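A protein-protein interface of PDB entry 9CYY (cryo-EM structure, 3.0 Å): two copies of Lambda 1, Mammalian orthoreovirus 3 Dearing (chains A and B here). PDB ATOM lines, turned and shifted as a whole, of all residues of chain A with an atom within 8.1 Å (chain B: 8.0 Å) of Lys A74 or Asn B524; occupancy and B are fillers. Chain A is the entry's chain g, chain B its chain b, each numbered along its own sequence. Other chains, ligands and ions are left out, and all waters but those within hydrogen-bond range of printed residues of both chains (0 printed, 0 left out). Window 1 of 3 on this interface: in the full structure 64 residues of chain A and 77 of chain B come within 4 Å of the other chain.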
ATOM      1  N   MET A  71       2.654  -9.253 -32.117  1.00  0.00           N
ATOM      2  CA  MET A  71       3.890  -9.738 -31.524  1.00  0.00           C
ATOM      3  C   MET A  71       4.656  -8.591 -30.869  1.00  0.00           C
ATOM      4  O   MET A  71       4.944  -7.585 -31.534  1.00  0.00           O
ATOM      5  CB  MET A  71       4.761 -10.404 -32.588  1.00  0.00           C
ATOM      6  CG  MET A  71       4.182 -11.672 -33.192  1.00  0.00           C
ATOM      7  SD  MET A  71       3.936 -12.983 -31.981  1.00  0.00           S
ATOM      8  CE  MET A  71       2.172 -12.880 -31.714  1.00  0.00           C
ATOM      9  N   PRO A  72       4.998  -8.697 -29.589  1.00  0.00           N
ATOM     10  CA  PRO A  72       5.890  -7.710 -28.976  1.00  0.00           C
ATOM     11  C   PRO A  72       7.306  -7.856 -29.513  1.00  0.00           C
ATOM     12  O   PRO A  72       7.708  -8.904 -30.022  1.00  0.00           O
ATOM     13  CB  PRO A  72       5.815  -8.042 -27.483  1.00  0.00           C
ATOM     14  CG  PRO A  72       5.447  -9.486 -27.444  1.00  0.00           C
ATOM     15  CD  PRO A  72       4.545  -9.711 -28.623  1.00  0.00           C
ATOM     16  N   MET A  73       8.065  -6.772 -29.402  1.00  0.00           N
ATOM     17  CA  MET A  73       9.425  -6.761 -29.912  1.00  0.00           C
ATOM     18  C   MET A  73      10.318  -7.685 -29.091  1.00  0.00           C
ATOM     19  O   MET A  73      10.065  -7.960 -27.915  1.00  0.00           O
ATOM     20  CB  MET A  73       9.994  -5.344 -29.907  1.00  0.00           C
ATOM     21  CG  MET A  73       9.343  -4.412 -30.911  1.00  0.00           C
ATOM     22  SD  MET A  73      10.179  -2.819 -31.028  1.00  0.00           S
ATOM     23  CE  MET A  73      10.763  -2.614 -29.349  1.00  0.00           C
ATOM     24  N   LYS A  74      11.378  -8.169 -29.733  1.00  0.00           N
ATOM     25  CA  LYS A  74      12.314  -9.059 -29.068  1.00  0.00           C
ATOM     26  C   LYS A  74      13.124  -8.299 -28.023  1.00  0.00           C
ATOM     27  O   LYS A  74      13.175  -7.068 -28.008  1.00  0.00           O
ATOM     28  CB  LYS A  74      13.251  -9.709 -30.085  1.00  0.00           C
ATOM     29  CG  LYS A  74      14.192  -8.732 -30.757  1.00  0.00           C
ATOM     30  CD  LYS A  74      15.027  -9.413 -31.825  1.00  0.00           C
ATOM     31  CE  LYS A  74      16.067 -10.329 -31.211  1.00  0.00           C
ATOM     32  NZ  LYS A  74      16.957 -10.924 -32.246  1.00  0.00           N
ATOM     33  N   ASN A  75      13.766  -9.056 -27.139  1.00  0.00           N
ATOM     34  CA  ASN A  75      14.544  -8.502 -26.038  1.00  0.00           C
ATOM     35  C   ASN A  75      15.999  -8.460 -26.491  1.00  0.00           C
ATOM     36  O   ASN A  75      16.575  -9.492 -26.850  1.00  0.00           O
ATOM     37  CB  ASN A  75      14.360  -9.344 -24.774  1.00  0.00           C
ATOM     38  CG  ASN A  75      15.219  -8.877 -23.600  1.00  0.00           C
ATOM     39  OD1 ASN A  75      16.268  -8.257 -23.767  1.00  0.00           O
ATOM     40  ND2 ASN A  75      14.761  -9.181 -22.392  1.00  0.00           N
ATOM     41  N   ASN A  76      16.588  -7.267 -26.472  1.00  0.00           N
ATOM     42  CA  ASN A  76      17.991  -7.076 -26.840  1.00  0.00           C
ATOM     43  C   ASN A  76      18.784  -6.862 -25.557  1.00  0.00           C
ATOM     44  O   ASN A  76      19.019  -5.733 -25.126  1.00  0.00           O
ATOM     45  CB  ASN A  76      18.140  -5.904 -27.799  1.00  0.00           C
ATOM     46  CG  ASN A  76      19.537  -5.791 -28.370  1.00  0.00           C
ATOM     47  OD1 ASN A  76      20.415  -6.593 -28.059  1.00  0.00           O
ATOM     48  ND2 ASN A  76      19.751  -4.786 -29.211  1.00  0.00           N
ATOM     49  N   ASP A  77      19.203  -7.963 -24.937  1.00  0.00           N
ATOM     50  CA  ASP A  77      19.928  -7.922 -23.675  1.00  0.00           C
ATOM     51  C   ASP A  77      21.434  -8.076 -23.848  1.00  0.00           C
ATOM     52  O   ASP A  77      22.146  -8.239 -22.852  1.00  0.00           O
ATOM     53  CB  ASP A  77      19.391  -8.994 -22.725  1.00  0.00           C
ATOM     54  CG  ASP A  77      19.588 -10.404 -23.254  1.00  0.00           C
ATOM     55  OD1 ASP A  77      20.105 -10.567 -24.381  1.00  0.00           O
ATOM     56  OD2 ASP A  77      19.223 -11.359 -22.537  1.00  0.00           O
ATOM     57  N   GLU A  78      21.931  -8.037 -25.080  1.00  0.00           N
ATOM     58  CA  GLU A  78      23.362  -8.167 -25.308  1.00  0.00           C
ATOM     59  C   GLU A  78      24.105  -6.967 -24.735  1.00  0.00           C
ATOM     60  O   GLU A  78      23.654  -5.825 -24.847  1.00  0.00           O
ATOM     61  CB  GLU A  78      23.648  -8.300 -26.803  1.00  0.00           C
ATOM     62  CG  GLU A  78      25.035  -8.825 -27.123  1.00  0.00           C
ATOM     63  CD  GLU A  78      25.055  -9.699 -28.362  1.00  0.00           C
ATOM     64  OE1 GLU A  78      26.148 -10.170 -28.741  1.00  0.00           O
ATOM     65  OE2 GLU A  78      23.978  -9.915 -28.956  1.00  0.00           O
ATOM     66  N   GLU A 101      24.570  -7.907 -38.059  1.00  0.00           N
ATOM     67  CA  GLU A 101      23.148  -7.946 -37.726  1.00  0.00           C
ATOM     68  C   GLU A 101      22.287  -7.457 -38.883  1.00  0.00           C
ATOM     69  O   GLU A 101      21.112  -7.828 -38.990  1.00  0.00           O
ATOM     70  CB  GLU A 101      22.894  -7.113 -36.472  1.00  0.00           C
ATOM     71  CG  GLU A 101      23.521  -7.699 -35.220  1.00  0.00           C
ATOM     72  CD  GLU A 101      23.282  -6.849 -33.992  1.00  0.00           C
ATOM     73  OE1 GLU A 101      22.734  -5.737 -34.138  1.00  0.00           O
ATOM     74  OE2 GLU A 101      23.641  -7.291 -32.881  1.00  0.00           O
ATOM     75  N   SER A 134      26.988  -0.925 -32.406  1.00  0.00           N
ATOM     76  CA  SER A 134      25.940  -1.750 -31.826  1.00  0.00           C
ATOM     77  C   SER A 134      26.485  -2.451 -30.594  1.00  0.00           C
ATOM     78  O   SER A 134      27.686  -2.706 -30.490  1.00  0.00           O
ATOM     79  CB  SER A 134      25.410  -2.780 -32.828  1.00  0.00           C
ATOM     80  OG  SER A 134      24.417  -3.597 -32.234  1.00  0.00           O
ATOM     81  N   ARG A 135      25.589  -2.764 -29.662  1.00  0.00           N
ATOM     82  CA  ARG A 135      26.001  -3.373 -28.404  1.00  0.00           C
ATOM     83  C   ARG A 135      26.596  -4.755 -28.642  1.00  0.00           C
ATOM     84  O   ARG A 135      26.133  -5.512 -29.499  1.00  0.00           O
ATOM     85  CB  ARG A 135      24.813  -3.469 -27.451  1.00  0.00           C
ATOM     86  CG  ARG A 135      24.350  -2.130 -26.912  1.00  0.00           C
ATOM     87  CD  ARG A 135      23.838  -2.261 -25.490  1.00  0.00           C
ATOM     88  NE  ARG A 135      22.540  -2.924 -25.424  1.00  0.00           N
ATOM     89  CZ  ARG A 135      21.406  -2.412 -25.883  1.00  0.00           C
ATOM     90  NH1 ARG A 135      21.359  -1.208 -26.429  1.00  0.00           N
ATOM     91  NH2 ARG A 135      20.288  -3.122 -25.783  1.00  0.00           N
ATOM     92  N   GLN B 518       7.974   4.836 -23.646  1.00  0.00           N
ATOM     93  CA  GLN B 518       8.313   5.023 -25.052  1.00  0.00           C
ATOM     94  C   GLN B 518       9.815   5.187 -25.240  1.00  0.00           C
ATOM     95  O   GLN B 518      10.391   4.647 -26.191  1.00  0.00           O
ATOM     96  CB  GLN B 518       7.569   6.234 -25.609  1.00  0.00           C
ATOM     97  CG  GLN B 518       8.008   6.642 -27.001  1.00  0.00           C
ATOM     98  CD  GLN B 518       7.643   5.619 -28.050  1.00  0.00           C
ATOM     99  OE1 GLN B 518       6.502   5.553 -28.498  1.00  0.00           O
ATOM    100  NE2 GLN B 518       8.610   4.801 -28.437  1.00  0.00           N
ATOM    101  N   ILE B 519      10.464   5.934 -24.346  1.00  0.00           N
ATOM    102  CA  ILE B 519      11.903   6.150 -24.454  1.00  0.00           C
ATOM    103  C   ILE B 519      12.656   4.836 -24.293  1.00  0.00           C
ATOM    104  O   ILE B 519      13.616   4.561 -25.022  1.00  0.00           O
ATOM    105  CB  ILE B 519      12.359   7.197 -23.422  1.00  0.00           C
ATOM    106  CG1 ILE B 519      11.834   8.580 -23.803  1.00  0.00           C
ATOM    107  CG2 ILE B 519      13.871   7.224 -23.319  1.00  0.00           C
ATOM    108  CD1 ILE B 519      12.259   9.674 -22.856  1.00  0.00           C
ATOM    109  N   ILE B 520      12.233   4.005 -23.339  1.00  0.00           N
ATOM    110  CA  ILE B 520      12.900   2.725 -23.108  1.00  0.00           C
ATOM    111  C   ILE B 520      12.822   1.848 -24.350  1.00  0.00           C
ATOM    112  O   ILE B 520      13.786   1.158 -24.702  1.00  0.00           O
ATOM    113  CB  ILE B 520      12.296   2.022 -21.881  1.00  0.00           C
ATOM    114  CG1 ILE B 520      12.342   2.944 -20.664  1.00  0.00           C
ATOM    115  CG2 ILE B 520      13.028   0.723 -21.596  1.00  0.00           C
ATOM    116  CD1 ILE B 520      13.701   3.024 -20.014  1.00  0.00           C
ATOM    117  N   ARG B 521      11.675   1.857 -25.032  1.00  0.00           N
ATOM    118  CA  ARG B 521      11.527   1.055 -26.241  1.00  0.00           C
ATOM    119  C   ARG B 521      12.516   1.488 -27.314  1.00  0.00           C
ATOM    120  O   ARG B 521      13.069   0.649 -28.033  1.00  0.00           O
ATOM    121  CB  ARG B 521      10.096   1.153 -26.764  1.00  0.00           C
ATOM    122  CG  ARG B 521       9.204   0.007 -26.331  1.00  0.00           C
ATOM    123  CD  ARG B 521       7.866   0.053 -27.041  1.00  0.00           C
ATOM    124  NE  ARG B 521       6.985   1.070 -26.479  1.00  0.00           N
ATOM    125  CZ  ARG B 521       6.078   0.839 -25.541  1.00  0.00           C
ATOM    126  NH1 ARG B 521       5.904  -0.370 -25.031  1.00  0.00           N
ATOM    127  NH2 ARG B 521       5.328   1.844 -25.102  1.00  0.00           N
ATOM    128  N   ILE B 522      12.748   2.795 -27.440  1.00  0.00           N
ATOM    129  CA  ILE B 522      13.686   3.295 -28.441  1.00  0.00           C
ATOM    130  C   ILE B 522      15.104   2.838 -28.121  1.00  0.00           C
ATOM    131  O   ILE B 522      15.862   2.446 -29.016  1.00  0.00           O
ATOM    132  CB  ILE B 522      13.589   4.827 -28.538  1.00  0.00           C
ATOM    133  CG1 ILE B 522      12.185   5.238 -28.980  1.00  0.00           C
ATOM    134  CG2 ILE B 522      14.635   5.368 -29.495  1.00  0.00           C
ATOM    135  CD1 ILE B 522      12.064   6.691 -29.364  1.00  0.00           C
ATOM    136  N   MET B 523      15.484   2.880 -26.843  1.00  0.00           N
ATOM    137  CA  MET B 523      16.831   2.475 -26.453  1.00  0.00           C
ATOM    138  C   MET B 523      17.073   0.998 -26.731  1.00  0.00           C
ATOM    139  O   MET B 523      18.218   0.575 -26.923  1.00  0.00           O
ATOM    140  CB  MET B 523      17.059   2.781 -24.974  1.00  0.00           C
ATOM    141  CG  MET B 523      17.076   4.256 -24.639  1.00  0.00           C
ATOM    142  SD  MET B 523      17.263   4.546 -22.872  1.00  0.00           S
ATOM    143  CE  MET B 523      18.960   4.041 -22.630  1.00  0.00           C
ATOM    144  N   ASN B 524      16.007   0.197 -26.754  1.00  0.00           N
ATOM    145  CA  ASN B 524      16.164  -1.245 -26.913  1.00  0.00           C
ATOM    146  C   ASN B 524      16.728  -1.604 -28.280  1.00  0.00           C
ATOM    147  O   ASN B 524      17.424  -2.616 -28.423  1.00  0.00           O
ATOM    148  CB  ASN B 524      14.826  -1.946 -26.694  1.00  0.00           C
ATOM    149  CG  ASN B 524      14.937  -3.451 -26.802  1.00  0.00           C
ATOM    150  OD1 ASN B 524      15.720  -4.079 -26.092  1.00  0.00           O
ATOM    151  ND2 ASN B 524      14.153  -4.039 -27.696  1.00  0.00           N
ATOM    152  N   ILE B 525      16.433  -0.796 -29.300  1.00  0.00           N
ATOM    153  CA  ILE B 525      16.827  -1.150 -30.661  1.00  0.00           C
ATOM    154  C   ILE B 525      18.344  -1.220 -30.778  1.00  0.00           C
ATOM    155  O   ILE B 525      18.900  -2.222 -31.241  1.00  0.00           O
ATOM    156  CB  ILE B 525      16.228  -0.153 -31.667  1.00  0.00           C
ATOM    157  CG1 ILE B 525      14.703  -0.227 -31.636  1.00  0.00           C
ATOM    158  CG2 ILE B 525      16.749  -0.434 -33.063  1.00  0.00           C
ATOM    159  CD1 ILE B 525      14.025   0.911 -32.354  1.00  0.00           C
ATOM    160  N   GLY B 526      19.032  -0.173 -30.340  1.00  0.00           N
ATOM    161  CA  GLY B 526      20.491  -0.199 -30.330  1.00  0.00           C
ATOM    162  C   GLY B 526      21.114  -0.458 -31.681  1.00  0.00           C
ATOM    163  O   GLY B 526      22.100  -1.200 -31.779  1.00  0.00           O
ATOM    164  N   ASN B 527      20.553   0.134 -32.736  1.00  0.00           N
ATOM    165  CA  ASN B 527      21.060  -0.027 -34.102  1.00  0.00           C
ATOM    166  C   ASN B 527      21.091  -1.492 -34.528  1.00  0.00           C
ATOM    167  O   ASN B 527      21.950  -1.907 -35.310  1.00  0.00           O
ATOM    168  CB  ASN B 527      22.445   0.606 -34.258  1.00  0.00           C
ATOM    169  CG  ASN B 527      22.435   2.093 -33.999  1.00  0.00           C
ATOM    170  OD1 ASN B 527      21.392   2.679 -33.723  1.00  0.00           O
ATOM    171  ND2 ASN B 527      23.603   2.716 -34.085  1.00  0.00           N
ATOM    172  N   ASN B 528      20.155  -2.289 -34.021  1.00  0.00           N
ATOM    173  CA  ASN B 528      20.042  -3.701 -34.372  1.00  0.00           C
ATOM    174  C   ASN B 528      18.914  -3.839 -35.386  1.00  0.00           C
ATOM    175  O   ASN B 528      17.744  -3.628 -35.054  1.00  0.00           O
ATOM    176  CB  ASN B 528      19.787  -4.555 -33.132  1.00  0.00           C
ATOM    177  CG  ASN B 528      19.890  -6.042 -33.411  1.00  0.00           C
ATOM    178  OD1 ASN B 528      19.866  -6.476 -34.561  1.00  0.00           O
ATOM    179  ND2 ASN B 528      20.015  -6.831 -32.351  1.00  0.00           N
ATOM    180  N   ALA B 529      19.269  -4.196 -36.622  1.00  0.00           N
ATOM    181  CA  ALA B 529      18.271  -4.291 -37.679  1.00  0.00           C
ATOM    182  C   ALA B 529      17.310  -5.450 -37.453  1.00  0.00           C
ATOM    183  O   ALA B 529      16.153  -5.384 -37.880  1.00  0.00           O
ATOM    184  CB  ALA B 529      18.955  -4.427 -39.036  1.00  0.00           C
ATOM    185  N   THR B 530      17.764  -6.515 -36.789  1.00  0.00           N
ATOM    186  CA  THR B 530      16.904  -7.670 -36.565  1.00  0.00           C
ATOM    187  C   THR B 530      15.767  -7.369 -35.599  1.00  0.00           C
ATOM    188  O   THR B 530      14.802  -8.137 -35.541  1.00  0.00           O
ATOM    189  CB  THR B 530      17.723  -8.847 -36.039  1.00  0.00           C
ATOM    190  OG1 THR B 530      18.522  -8.416 -34.931  1.00  0.00           O
ATOM    191  CG2 THR B 530      18.630  -9.386 -37.130  1.00  0.00           C
ATOM    192  N   VAL B 531      15.859  -6.274 -34.842  1.00  0.00           N
ATOM    193  CA  VAL B 531      14.787  -5.886 -33.930  1.00  0.00           C
ATOM    194  C   VAL B 531      13.709  -5.063 -34.618  1.00  0.00           C
ATOM    195  O   VAL B 531      12.533  -5.151 -34.231  1.00  0.00           O
ATOM    196  CB  VAL B 531      15.364  -5.102 -32.733  1.00  0.00           C
ATOM    197  CG1 VAL B 531      14.275  -4.757 -31.733  1.00  0.00           C
ATOM    198  CG2 VAL B 531      16.466  -5.901 -32.064  1.00  0.00           C
ATOM    199  N   ILE B 532      14.060  -4.293 -35.644  1.00  0.00           N
ATOM    200  CA  ILE B 532      13.129  -3.357 -36.261  1.00  0.00           C
ATOM    201  C   ILE B 532      12.534  -3.977 -37.519  1.00  0.00           C
ATOM    202  O   ILE B 532      11.505  -3.520 -38.025  1.00  0.00           O
ATOM    203  CB  ILE B 532      13.833  -2.023 -36.574  1.00  0.00           C
ATOM    204  CG1 ILE B 532      12.823  -0.951 -36.982  1.00  0.00           C
ATOM    205  CG2 ILE B 532      14.875  -2.212 -37.661  1.00  0.00           C
ATOM    206  CD1 ILE B 532      11.712  -0.749 -35.983  1.00  0.00           C
ATOM    207  N   GLN B 533      13.177  -5.024 -38.033  1.00  0.00           N
ATOM    208  CA  GLN B 533      12.694  -5.657 -39.258  1.00  0.00           C
ATOM    209  C   GLN B 533      11.306  -6.272 -39.121  1.00  0.00           C
ATOM    210  O   GLN B 533      10.462  -6.027 -40.001  1.00  0.00           O
ATOM    211  CB  GLN B 533      13.710  -6.697 -39.736  1.00  0.00           C
ATOM    212  CG  GLN B 533      13.388  -7.291 -41.095  1.00  0.00           C
ATOM    213  CD  GLN B 533      12.645  -8.603 -40.992  1.00  0.00           C
ATOM    214  OE1 GLN B 533      12.503  -9.165 -39.908  1.00  0.00           O
ATOM    215  NE2 GLN B 533      12.159  -9.099 -42.123  1.00  0.00           N
ATOM    216  N   PRO B 534      10.999  -7.076 -38.093  1.00  0.00           N
ATOM    217  CA  PRO B 534       9.685  -7.748 -38.080  1.00  0.00           C
ATOM    218  C   PRO B 534       8.495  -6.801 -38.071  1.00  0.00           C
ATOM    219  O   PRO B 534       7.480  -7.094 -38.713  1.00  0.00           O
ATOM    220  CB  PRO B 534       9.750  -8.595 -36.802  1.00  0.00           C
ATOM    221  CG  PRO B 534      11.192  -8.812 -36.573  1.00  0.00           C
ATOM    222  CD  PRO B 534      11.833  -7.523 -36.965  1.00  0.00           C
ATOM    223  N   VAL B 535       8.585  -5.671 -37.368  1.00  0.00           N
ATOM    224  CA  VAL B 535       7.409  -4.820 -37.201  1.00  0.00           C
ATOM    225  C   VAL B 535       7.019  -4.175 -38.525  1.00  0.00           C
ATOM    226  O   VAL B 535       5.834  -4.059 -38.854  1.00  0.00           O
ATOM    227  CB  VAL B 535       7.644  -3.772 -36.096  1.00  0.00           C
ATOM    228  CG1 VAL B 535       7.811  -4.458 -34.753  1.00  0.00           C
ATOM    229  CG2 VAL B 535       8.851  -2.919 -36.401  1.00  0.00           C
ATOM    230  N   ASP B 981       9.777 -10.604 -20.086  1.00  0.00           N
ATOM    231  CA  ASP B 981      10.266  -9.846 -21.230  1.00  0.00           C
ATOM    232  C   ASP B 981      11.060  -8.650 -20.718  1.00  0.00           C
ATOM    233  O   ASP B 981      11.421  -8.576 -19.539  1.00  0.00           O
ATOM    234  CB  ASP B 981       9.112  -9.412 -22.144  1.00  0.00           C
ATOM    235  CG  ASP B 981       8.467 -10.576 -22.866  1.00  0.00           C
ATOM    236  OD1 ASP B 981       9.164 -11.576 -23.133  1.00  0.00           O
ATOM    237  OD2 ASP B 981       7.262 -10.488 -23.179  1.00  0.00           O
ATOM    238  N   MET B 982      11.339  -7.717 -21.625  1.00  0.00           N
ATOM    239  CA  MET B 982      12.184  -6.573 -21.307  1.00  0.00           C
ATOM    240  C   MET B 982      11.592  -5.730 -20.188  1.00  0.00           C
ATOM    241  O   MET B 982      10.404  -5.400 -20.191  1.00  0.00           O
ATOM    242  CB  MET B 982      12.380  -5.706 -22.547  1.00  0.00           C
ATOM    243  CG  MET B 982      13.290  -4.518 -22.315  1.00  0.00           C
ATOM    244  SD  MET B 982      13.515  -3.532 -23.799  1.00  0.00           S
ATOM    245  CE  MET B 982      11.905  -2.761 -23.933  1.00  0.00           C
ATOM    246  N   LEU B 983      12.440  -5.382 -19.220  1.00  0.00           N
ATOM    247  CA  LEU B 983      12.079  -4.412 -18.186  1.00  0.00           C
ATOM    248  C   LEU B 983      13.396  -3.844 -17.645  1.00  0.00           C
ATOM    249  O   LEU B 983      14.104  -4.517 -16.897  1.00  0.00           O
ATOM    250  CB  LEU B 983      11.248  -5.033 -17.084  1.00  0.00           C
ATOM    251  CG  LEU B 983      10.789  -4.067 -15.993  1.00  0.00           C
ATOM    252  CD1 LEU B 983       9.809  -3.059 -16.558  1.00  0.00           C
ATOM    253  CD2 LEU B 983      10.172  -4.820 -14.830  1.00  0.00           C
ATOM    254  N   GLU B 985      16.156  -3.415 -19.075  1.00  0.00           N
ATOM    255  CA  GLU B 985      17.396  -3.951 -19.637  1.00  0.00           C
ATOM    256  C   GLU B 985      18.219  -2.910 -20.386  1.00  0.00           C
ATOM    257  O   GLU B 985      19.447  -2.879 -20.193  1.00  0.00           O
ATOM    258  CB  GLU B 985      17.088  -5.159 -20.530  1.00  0.00           C
ATOM    259  CG  GLU B 985      17.037  -6.483 -19.788  1.00  0.00           C
ATOM    260  CD  GLU B 985      15.697  -6.738 -19.136  1.00  0.00           C
ATOM    261  OE1 GLU B 985      14.776  -5.919 -19.329  1.00  0.00           O
ATOM    262  OE2 GLU B 985      15.562  -7.758 -18.430  1.00  0.00           O
ATOM    263  N   PRO B 986      17.650  -2.054 -21.242  1.00  0.00           N
ATOM    264  CA  PRO B 986      18.492  -1.064 -21.936  1.00  0.00           C
ATOM    265  C   PRO B 986      19.182  -0.085 -21.007  1.00  0.00           C
ATOM    266  O   PRO B 986      20.174   0.534 -21.412  1.00  0.00           O
ATOM    267  CB  PRO B 986      17.501  -0.349 -22.862  1.00  0.00           C
ATOM    268  CG  PRO B 986      16.410  -1.326 -23.065  1.00  0.00           C
ATOM    269  CD  PRO B 986      16.268  -2.024 -21.753  1.00  0.00           C
ATOM    270  N   LEU B 987      18.701   0.080 -19.778  1.00  0.00           N
ATOM    271  CA  LEU B 987      19.309   1.010 -18.839  1.00  0.00           C
ATOM    272  C   LEU B 987      20.585   0.473 -18.208  1.00  0.00           C
ATOM    273  O   LEU B 987      21.285   1.229 -17.527  1.00  0.00           O
ATOM    274  CB  LEU B 987      18.311   1.372 -17.739  1.00  0.00           C
ATOM    275  CG  LEU B 987      17.263   2.421 -18.104  1.00  0.00           C
ATOM    276  CD1 LEU B 987      16.562   2.919 -16.857  1.00  0.00           C
ATOM    277  CD2 LEU B 987      17.904   3.571 -18.857  1.00  0.00           C
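Of chain B, only Asn B524 (3.2 Å), Thr B530 (3.9 Å) and Val B531 (3.8 Å) come within 4 Å of Lys A74.
Of the printed residues of chain A, Asn B524 touches Lys A74 (3.2 Å), Asn A76 (3.3 Å) and Arg A135 (3.9 Å).
Printed residues of chain B within 4 Å of Asn A76: Asn B524 (3.3 Å), Ile B525 (3.4 Å) and Asn B528 (3.8 Å).
Of the printed residues of chain A, Ile B525 touches Asn A76 (3.4 Å).
Printed residues of chain B within 4 Å of Arg A135: Met B523 and Asn B524.
Of the printed residues of chain B, Glu A101 touches Asn B528 (3.0 Å) and Thr B530 (3.5 Å).
Of the printed residues of chain A, Met B523 touches Arg A135.
The nearest residue of chain A that does not touch Asn B524 is Met A73 (4.03 Å).
Among the printed residues, pairs that only touch across the chains: Lys A74 with Thr B530 (3.9 Å), Lys A74 with Val B531 (3.8 Å), Asn A75 with Met B982 (3.8 Å), Asn A76 with Asn B528 (3.8 Å), Glu A101 with Thr B530 (3.5 Å), Arg A135 with Met B523 (3.6 Å) and Arg A135 with Asn B524 (3.9 Å).
Of the 11 printed residues of chain A, 6 touch a printed residue of chain B.
Of the 24 printed residues of chain B, 8 touch a printed residue of chain A.
Hydrophobic or aromatic side chains of chain B within 4 Å of the printed part of chain A: Val B531.
Among the printed residues, no Asp or Glu carboxylate lies within 4 Å of a Lys or Arg side-chain nitrogen of the other chain.
ND2 of Asn B524 lies within hydrogen-bond range of O of Lys A74 (3.2 Å).
The backbone carbonyl oxygen (O) of Asn B524 sits at hydrogen-bond distance from the side-chain amide nitrogen (ND2) of Asn A76 (3.3 Å).
The backbone carbonyl oxygen of Ile B525 is in hydrogen-bond range of the side-chain amide nitrogen of Asn A76 (3.4 Å).
The backbone carbonyl oxygen of Gly B526 is in hydrogen-bond range of the side-chain hydroxyl of Ser A134, at 3.4 Å.
OD1 of Asn B528 lies close to OE1 of Glu A101.
No position is printed for both chains.
Of the 12 pairs that touch across the chains among the printed residues, none has its exchanged pair printed and touching as well.
The side-chain amide oxygen of Asn B524 lies close to the side-chain sulfur of Met B982.
The side-chain amide oxygen of Asn B528 sits at hydrogen-bond distance from the backbone NH of Thr B530 (3.1 Å).
The backbone NH of Asp A77 lies within hydrogen-bond range of the side-chain amide oxygen of Asn A75 (3.2 Å).
NH2 of Arg A135 lies within hydrogen-bond range of O of Asn A76, at 3.0 Å.
The guanidinium group of Arg A135 is in hydrogen-bond range of the backbone carbonyl oxygen of Glu A78 (3.2 Å).
The side-chain carboxylate (OE1) of Glu A101 lies within hydrogen-bond range of the side-chain hydroxyl (OG) of Ser A134 (3.3 Å).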
